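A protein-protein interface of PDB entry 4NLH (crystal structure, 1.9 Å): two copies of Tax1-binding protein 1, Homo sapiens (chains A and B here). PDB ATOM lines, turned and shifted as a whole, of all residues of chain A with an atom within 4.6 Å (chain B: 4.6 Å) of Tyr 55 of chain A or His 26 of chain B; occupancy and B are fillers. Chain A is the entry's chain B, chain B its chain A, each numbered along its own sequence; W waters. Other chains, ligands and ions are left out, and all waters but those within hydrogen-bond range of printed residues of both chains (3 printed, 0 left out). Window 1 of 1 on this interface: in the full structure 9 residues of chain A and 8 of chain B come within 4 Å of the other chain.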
ATOM      1  N   ILE A  43     -27.837   8.512   3.809  1.00  0.00           N
ATOM      2  CA  ILE A  43     -28.974   9.195   3.214  1.00  0.00           C
ATOM      3  C   ILE A  43     -28.457  10.533   2.671  1.00  0.00           C
ATOM      4  O   ILE A  43     -28.025  11.405   3.442  1.00  0.00           O
ATOM      5  CB  ILE A  43     -30.104   9.361   4.236  1.00  0.00           C
ATOM      6  CG1 ILE A  43     -30.615   7.972   4.671  1.00  0.00           C
ATOM      7  CG2 ILE A  43     -31.239  10.182   3.665  1.00  0.00           C
ATOM      8  CD1 ILE A  43     -31.798   8.009   5.611  1.00  0.00           C
ATOM      9  N   ASP A  53     -21.035  14.654   1.679  1.00  0.00           N
ATOM     10  CA  ASP A  53     -22.291  15.407   1.664  1.00  0.00           C
ATOM     11  C   ASP A  53     -23.493  14.645   2.238  1.00  0.00           C
ATOM     12  O   ASP A  53     -24.629  14.912   1.846  1.00  0.00           O
ATOM     13  CB  ASP A  53     -22.620  15.871   0.233  1.00  0.00           C
ATOM     14  CG  ASP A  53     -21.709  16.988  -0.251  1.00  0.00           C
ATOM     15  OD1 ASP A  53     -21.073  17.643   0.596  1.00  0.00           O
ATOM     16  OD2 ASP A  53     -21.643  17.220  -1.477  1.00  0.00           O
ATOM     17  N   TYR A  54     -23.261  13.714   3.162  1.00  0.00           N
ATOM     18  CA  TYR A  54     -24.365  12.910   3.713  1.00  0.00           C
ATOM     19  C   TYR A  54     -25.195  13.670   4.744  1.00  0.00           C
ATOM     20  O   TYR A  54     -24.703  14.601   5.379  1.00  0.00           O
ATOM     21  CB  TYR A  54     -23.858  11.595   4.321  1.00  0.00           C
ATOM     22  CG  TYR A  54     -22.967  11.744   5.546  1.00  0.00           C
ATOM     23  CD1 TYR A  54     -23.514  11.870   6.825  1.00  0.00           C
ATOM     24  CD2 TYR A  54     -21.587  11.713   5.426  1.00  0.00           C
ATOM     25  CE1 TYR A  54     -22.710  11.987   7.940  1.00  0.00           C
ATOM     26  CE2 TYR A  54     -20.771  11.834   6.531  1.00  0.00           C
ATOM     27  CZ  TYR A  54     -21.335  11.971   7.788  1.00  0.00           C
ATOM     28  OH  TYR A  54     -20.511  12.089   8.889  1.00  0.00           O
ATOM     29  N   TYR A  55     -26.447  13.262   4.910  1.00  0.00           N
ATOM     30  CA  TYR A  55     -27.314  13.850   5.918  1.00  0.00           C
ATOM     31  C   TYR A  55     -27.153  13.069   7.217  1.00  0.00           C
ATOM     32  O   TYR A  55     -27.018  13.648   8.304  1.00  0.00           O
ATOM     33  CB  TYR A  55     -28.772  13.811   5.444  1.00  0.00           C
ATOM     34  CG  TYR A  55     -29.694  14.561   6.359  1.00  0.00           C
ATOM     35  CD1 TYR A  55     -30.304  13.927   7.421  1.00  0.00           C
ATOM     36  CD2 TYR A  55     -29.910  15.913   6.186  1.00  0.00           C
ATOM     37  CE1 TYR A  55     -31.127  14.615   8.269  1.00  0.00           C
ATOM     38  CE2 TYR A  55     -30.739  16.611   7.024  1.00  0.00           C
ATOM     39  CZ  TYR A  55     -31.343  15.956   8.062  1.00  0.00           C
ATOM     40  OH  TYR A  55     -32.165  16.645   8.920  1.00  0.00           O
ATOM     41  N   THR A  56     -27.168  11.745   7.087  1.00  0.00           N
ATOM     42  CA  THR A  56     -26.879  10.841   8.185  1.00  0.00           C
ATOM     43  C   THR A  56     -26.377   9.554   7.547  1.00  0.00           C
ATOM     44  O   THR A  56     -26.551   9.355   6.326  1.00  0.00           O
ATOM     45  CB  THR A  56     -28.125  10.551   9.049  1.00  0.00           C
ATOM     46  OG1 THR A  56     -27.743   9.805  10.214  1.00  0.00           O
ATOM     47  CG2 THR A  56     -29.166   9.749   8.271  1.00  0.00           C
ATOM     48  N   TYR A  82     -32.766  10.725  13.468  1.00  0.00           N
ATOM     49  CA  TYR A  82     -31.650  11.128  12.607  1.00  0.00           C
ATOM     50  C   TYR A  82     -32.134  11.419  11.191  1.00  0.00           C
ATOM     51  O   TYR A  82     -31.344  11.813  10.319  1.00  0.00           O
ATOM     52  CB  TYR A  82     -30.594  10.019  12.567  1.00  0.00           C
ATOM     53  CG  TYR A  82     -29.939   9.732  13.899  1.00  0.00           C
ATOM     54  CD1 TYR A  82     -29.636  10.761  14.774  1.00  0.00           C
ATOM     55  CD2 TYR A  82     -29.613   8.422  14.271  1.00  0.00           C
ATOM     56  CE1 TYR A  82     -29.035  10.517  15.990  1.00  0.00           C
ATOM     57  CE2 TYR A  82     -29.008   8.158  15.501  1.00  0.00           C
ATOM     58  CZ  TYR A  82     -28.729   9.213  16.347  1.00  0.00           C
ATOM     59  OH  TYR A  82     -28.132   8.993  17.555  1.00  0.00           O
ATOM     60  N   LEU A  83     -33.432  11.220  10.945  1.00  0.00           N
ATOM     61  CA  LEU A  83     -33.962  11.385   9.590  1.00  0.00           C
ATOM     62  C   LEU A  83     -34.356  12.839   9.319  1.00  0.00           C
ATOM     63  O   LEU A  83     -34.652  13.594  10.252  1.00  0.00           O
ATOM     64  CB  LEU A  83     -35.169  10.458   9.364  1.00  0.00           C
ATOM     65  CG  LEU A  83     -35.006   8.945   9.400  1.00  0.00           C
ATOM     66  CD1 LEU A  83     -36.339   8.280   9.111  1.00  0.00           C
ATOM     67  CD2 LEU A  83     -33.990   8.477   8.405  1.00  0.00           C
ATOM     68  N   PRO A  84     -34.360  13.254   8.043  1.00  0.00           N
ATOM     69  CA  PRO A  84     -34.871  14.614   7.825  1.00  0.00           C
ATOM     70  C   PRO A  84     -36.353  14.750   8.164  1.00  0.00           C
ATOM     71  O   PRO A  84     -37.061  13.752   8.374  1.00  0.00           O
ATOM     72  CB  PRO A  84     -34.669  14.838   6.323  1.00  0.00           C
ATOM     73  CG  PRO A  84     -33.630  13.825   5.905  1.00  0.00           C
ATOM     74  CD  PRO A  84     -33.855  12.640   6.799  1.00  0.00           C
ATOM     75  N   TYR A  91     -34.200  13.005  -1.253  1.00  0.00           N
ATOM     76  CA  TYR A  91     -33.054  12.272  -0.728  1.00  0.00           C
ATOM     77  C   TYR A  91     -32.933  10.923  -1.434  1.00  0.00           C
ATOM     78  O   TYR A  91     -33.900  10.438  -2.023  1.00  0.00           O
ATOM     79  CB  TYR A  91     -33.204  12.055   0.782  1.00  0.00           C
ATOM     80  CG  TYR A  91     -33.147  13.332   1.584  1.00  0.00           C
ATOM     81  CD1 TYR A  91     -31.934  13.835   2.044  1.00  0.00           C
ATOM     82  CD2 TYR A  91     -34.302  14.038   1.879  1.00  0.00           C
ATOM     83  CE1 TYR A  91     -31.877  15.012   2.771  1.00  0.00           C
ATOM     84  CE2 TYR A  91     -34.258  15.200   2.605  1.00  0.00           C
ATOM     85  CZ  TYR A  91     -33.047  15.685   3.045  1.00  0.00           C
ATOM     86  OH  TYR A  91     -33.029  16.857   3.763  1.00  0.00           O
ATOM     87  N   ILE B   9     -28.524  29.072  10.250  1.00  0.00           N
ATOM     88  CA  ILE B   9     -29.858  28.593  10.623  1.00  0.00           C
ATOM     89  C   ILE B   9     -29.787  27.132  10.977  1.00  0.00           C
ATOM     90  O   ILE B   9     -29.365  26.326  10.142  1.00  0.00           O
ATOM     91  CB  ILE B   9     -30.805  28.700   9.436  1.00  0.00           C
ATOM     92  CG1 ILE B   9     -30.781  30.127   8.886  1.00  0.00           C
ATOM     93  CG2 ILE B   9     -32.231  28.300   9.827  1.00  0.00           C
ATOM     94  CD1 ILE B   9     -31.385  31.107   9.831  1.00  0.00           C
ATOM     95  N   PHE B  10     -30.213  26.769  12.187  1.00  0.00           N
ATOM     96  CA  PHE B  10     -30.212  25.363  12.578  1.00  0.00           C
ATOM     97  C   PHE B  10     -31.465  24.707  12.043  1.00  0.00           C
ATOM     98  O   PHE B  10     -32.535  25.320  12.051  1.00  0.00           O
ATOM     99  CB  PHE B  10     -30.087  25.241  14.084  1.00  0.00           C
ATOM    100  CG  PHE B  10     -28.703  25.558  14.564  1.00  0.00           C
ATOM    101  CD1 PHE B  10     -27.728  24.578  14.574  1.00  0.00           C
ATOM    102  CD2 PHE B  10     -28.348  26.858  14.894  1.00  0.00           C
ATOM    103  CE1 PHE B  10     -26.435  24.869  14.965  1.00  0.00           C
ATOM    104  CE2 PHE B  10     -27.038  27.163  15.304  1.00  0.00           C
ATOM    105  CZ  PHE B  10     -26.092  26.166  15.341  1.00  0.00           C
ATOM    106  N   GLN B  11     -31.317  23.494  11.520  1.00  0.00           N
ATOM    107  CA  GLN B  11     -32.394  22.871  10.755  1.00  0.00           C
ATOM    108  C   GLN B  11     -32.881  21.616  11.447  1.00  0.00           C
ATOM    109  O   GLN B  11     -32.079  20.896  12.078  1.00  0.00           O
ATOM    110  CB  GLN B  11     -31.913  22.521   9.344  1.00  0.00           C
ATOM    111  CG  GLN B  11     -31.248  23.682   8.604  1.00  0.00           C
ATOM    112  CD  GLN B  11     -32.269  24.649   8.021  1.00  0.00           C
ATOM    113  OE1 GLN B  11     -33.464  24.356   7.977  1.00  0.00           O
ATOM    114  NE2 GLN B  11     -31.807  25.805   7.583  1.00  0.00           N
ATOM    115  N   ASN B  12     -34.189  21.360  11.329  1.00  0.00           N
ATOM    116  CA  ASN B  12     -34.825  20.142  11.844  1.00  0.00           C
ATOM    117  C   ASN B  12     -34.512  19.876  13.314  1.00  0.00           C
ATOM    118  O   ASN B  12     -34.247  18.728  13.713  1.00  0.00           O
ATOM    119  CB  ASN B  12     -34.438  18.923  10.984  1.00  0.00           C
ATOM    120  CG  ASN B  12     -35.246  17.671  11.331  1.00  0.00           C
ATOM    121  OD1 ASN B  12     -36.412  17.759  11.747  1.00  0.00           O
ATOM    122  ND2 ASN B  12     -34.624  16.504  11.179  1.00  0.00           N
ATOM    123  N   GLU B  24     -27.207  14.472  16.070  1.00  0.00           N
ATOM    124  CA  GLU B  24     -26.721  15.004  14.815  1.00  0.00           C
ATOM    125  C   GLU B  24     -27.319  16.390  14.613  1.00  0.00           C
ATOM    126  O   GLU B  24     -28.541  16.560  14.424  1.00  0.00           O
ATOM    127  CB  GLU B  24     -27.058  14.037  13.674  1.00  0.00           C
ATOM    128  CG  GLU B  24     -26.254  12.729  13.790  1.00  0.00           C
ATOM    129  CD  GLU B  24     -26.676  11.649  12.807  1.00  0.00           C
ATOM    130  OE1 GLU B  24     -27.373  11.959  11.830  1.00  0.00           O
ATOM    131  OE2 GLU B  24     -26.299  10.475  13.016  1.00  0.00           O
ATOM    132  N   CYS B  25     -26.444  17.382  14.666  1.00  0.00           N
ATOM    133  CA  CYS B  25     -26.848  18.778  14.579  1.00  0.00           C
ATOM    134  C   CYS B  25     -26.718  19.309  13.143  1.00  0.00           C
ATOM    135  O   CYS B  25     -25.619  19.290  12.554  1.00  0.00           O
ATOM    136  CB  CYS B  25     -25.946  19.572  15.532  1.00  0.00           C
ATOM    137  SG  CYS B  25     -26.157  21.340  15.422  1.00  0.00           S
ATOM    138  N   HIS B  26     -27.829  19.782  12.579  1.00  0.00           N
ATOM    139  CA  HIS B  26     -27.847  20.208  11.189  1.00  0.00           C
ATOM    140  C   HIS B  26     -28.008  21.702  11.147  1.00  0.00           C
ATOM    141  O   HIS B  26     -28.858  22.250  11.852  1.00  0.00           O
ATOM    142  CB  HIS B  26     -29.038  19.577  10.484  1.00  0.00           C
ATOM    143  CG  HIS B  26     -28.926  18.099  10.332  1.00  0.00           C
ATOM    144  ND1 HIS B  26     -28.260  17.509   9.279  1.00  0.00           N
ATOM    145  CD2 HIS B  26     -29.373  17.089  11.117  1.00  0.00           C
ATOM    146  CE1 HIS B  26     -28.318  16.194   9.414  1.00  0.00           C
ATOM    147  NE2 HIS B  26     -28.985  15.915  10.515  1.00  0.00           N
ATOM    148  N   TYR B  27     -27.209  22.369  10.328  1.00  0.00           N
ATOM    149  CA  TYR B  27     -27.333  23.814  10.214  1.00  0.00           C
ATOM    150  C   TYR B  27     -26.981  24.239   8.816  1.00  0.00           C
ATOM    151  O   TYR B  27     -26.315  23.488   8.095  1.00  0.00           O
ATOM    152  CB  TYR B  27     -26.449  24.534  11.242  1.00  0.00           C
ATOM    153  CG  TYR B  27     -24.992  24.096  11.297  1.00  0.00           C
ATOM    154  CD1 TYR B  27     -24.627  22.892  11.896  1.00  0.00           C
ATOM    155  CD2 TYR B  27     -23.988  24.914  10.802  1.00  0.00           C
ATOM    156  CE1 TYR B  27     -23.298  22.503  11.960  1.00  0.00           C
ATOM    157  CE2 TYR B  27     -22.653  24.545  10.882  1.00  0.00           C
ATOM    158  CZ  TYR B  27     -22.324  23.329  11.475  1.00  0.00           C
ATOM    159  OH  TYR B  27     -21.017  22.933  11.549  1.00  0.00           O
ATOM    160  N   CYS B  74     -24.579  21.758   6.655  1.00  0.00           N
ATOM    161  CA  CYS B  74     -23.523  21.167   7.470  1.00  0.00           C
ATOM    162  C   CYS B  74     -24.155  20.264   8.496  1.00  0.00           C
ATOM    163  O   CYS B  74     -25.356  20.396   8.799  1.00  0.00           O
ATOM    164  CB  CYS B  74     -22.768  22.259   8.217  1.00  0.00           C
ATOM    165  SG  CYS B  74     -22.196  23.622   7.178  1.00  0.00           S
ATOM    166  N   VAL B  75     -23.348  19.367   9.062  1.00  0.00           N
ATOM    167  CA  VAL B  75     -23.831  18.472  10.098  1.00  0.00           C
ATOM    168  C   VAL B  75     -22.688  18.191  11.085  1.00  0.00           C
ATOM    169  O   VAL B  75     -21.524  18.097  10.695  1.00  0.00           O
ATOM    170  CB  VAL B  75     -24.424  17.180   9.480  1.00  0.00           C
ATOM    171  CG1 VAL B  75     -23.368  16.421   8.706  1.00  0.00           C
ATOM    172  CG2 VAL B  75     -25.044  16.293  10.551  1.00  0.00           C
HETATM  173  O   HOH W   1     -25.222  13.140  10.381  1.00  0.00           O
HETATM  174  O   HOH W   2     -24.968   9.536  11.125  1.00  0.00           O
HETATM  175  O   HOH W   3     -29.435  13.460  11.557  1.00  0.00           O
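Water W2 bridges the side-chain carboxylate of Glu 24 of chain B (2.5 Å) and the side-chain hydroxyl of Thr 56 of chain A (2.9 Å).
Water W3 lies within hydrogen-bond range of the side-chain carboxylate of Glu 24 of chain B (2.6 Å), a ring nitrogen (NE2) of His 26 of chain B (2.7 Å) and the backbone carbonyl oxygen of Tyr 82 of chain A (2.8 Å).
Water W1 lies within hydrogen-bond range of the backbone carbonyl oxygen of Tyr 55 of chain A and the side-chain carboxylate of Glu 24 of chain B.
The side-chain carboxylate (OE1) of Glu 24 of chain B sits at hydrogen-bond distance from the side-chain hydroxyl (OG1) of Thr 56 of chain A (2.7 Å).
The side-chain amide nitrogen of Asn 12 of chain B is in hydrogen-bond range of the side-chain hydroxyl of Tyr 55 of chain A, at 3.3 Å.
The side-chain amide nitrogen (ND2) of Asn 12 of chain B sits at hydrogen-bond distance from the backbone carbonyl oxygen (O) of Leu 83 of chain A (3.1 Å).
No position is printed for both chains.
Of the 8 pairs that touch across the chains among the printed residues, none has its exchanged pair printed and touching as well.
O of Tyr 55 of chain A touches OE1 of Glu 24 of chain B, 3.9 Å away.
Tyr 55 of chain A touches His 26 of chain B (O to CE1, 3.1 Å).
Tyr 55 of chain A touches Val 75 of chain B (O to CG2, 3.99 Å).
CD1 of Tyr 82 of chain A touches CD of Glu 24 of chain B (3.7 Å).
CA of Pro 84 of chain A touches ND2 of Asn 12 of chain B, 3.9 Å away.
Among the printed residues, 8 pairs touch across the chains.
Printed residues of chain B within 4 Å of Tyr 55 of chain A: Asn 12, Glu 24, His 26 and Val 75.
His 26 of chain B touches just one residue of chain A: Tyr 55 (3.1 Å).
Of the printed residues of chain A, Asn 12 of chain B touches Tyr 55 (3.3 Å), Leu 83 (3.1 Å) and Pro 84 (3.9 Å).
Printed residues of chain B within 4 Å of Thr 56 of chain A: Glu 24 (2.7 Å).
Printed residues of chain B within 4 Å of Tyr 82 of chain A: Glu 24 (3.7 Å).
The nearest printed residue of chain A that does not touch His 26 of chain B is Tyr 82 of chain A (4.7 Å).
The backbone NH of Ile 43 of chain A lies within hydrogen-bond range of the backbone carbonyl oxygen of Thr 56 of chain A, at 2.9 Å.
The backbone NH of Gln 11 of chain B lies within hydrogen-bond range of the backbone carbonyl oxygen of His 26 of chain B (2.8 Å).
The backbone carbonyl oxygen (O) of Ile 43 of chain A is in hydrogen-bond range of the backbone NH (N) of Tyr 55 of chain A, at 2.8 Å.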
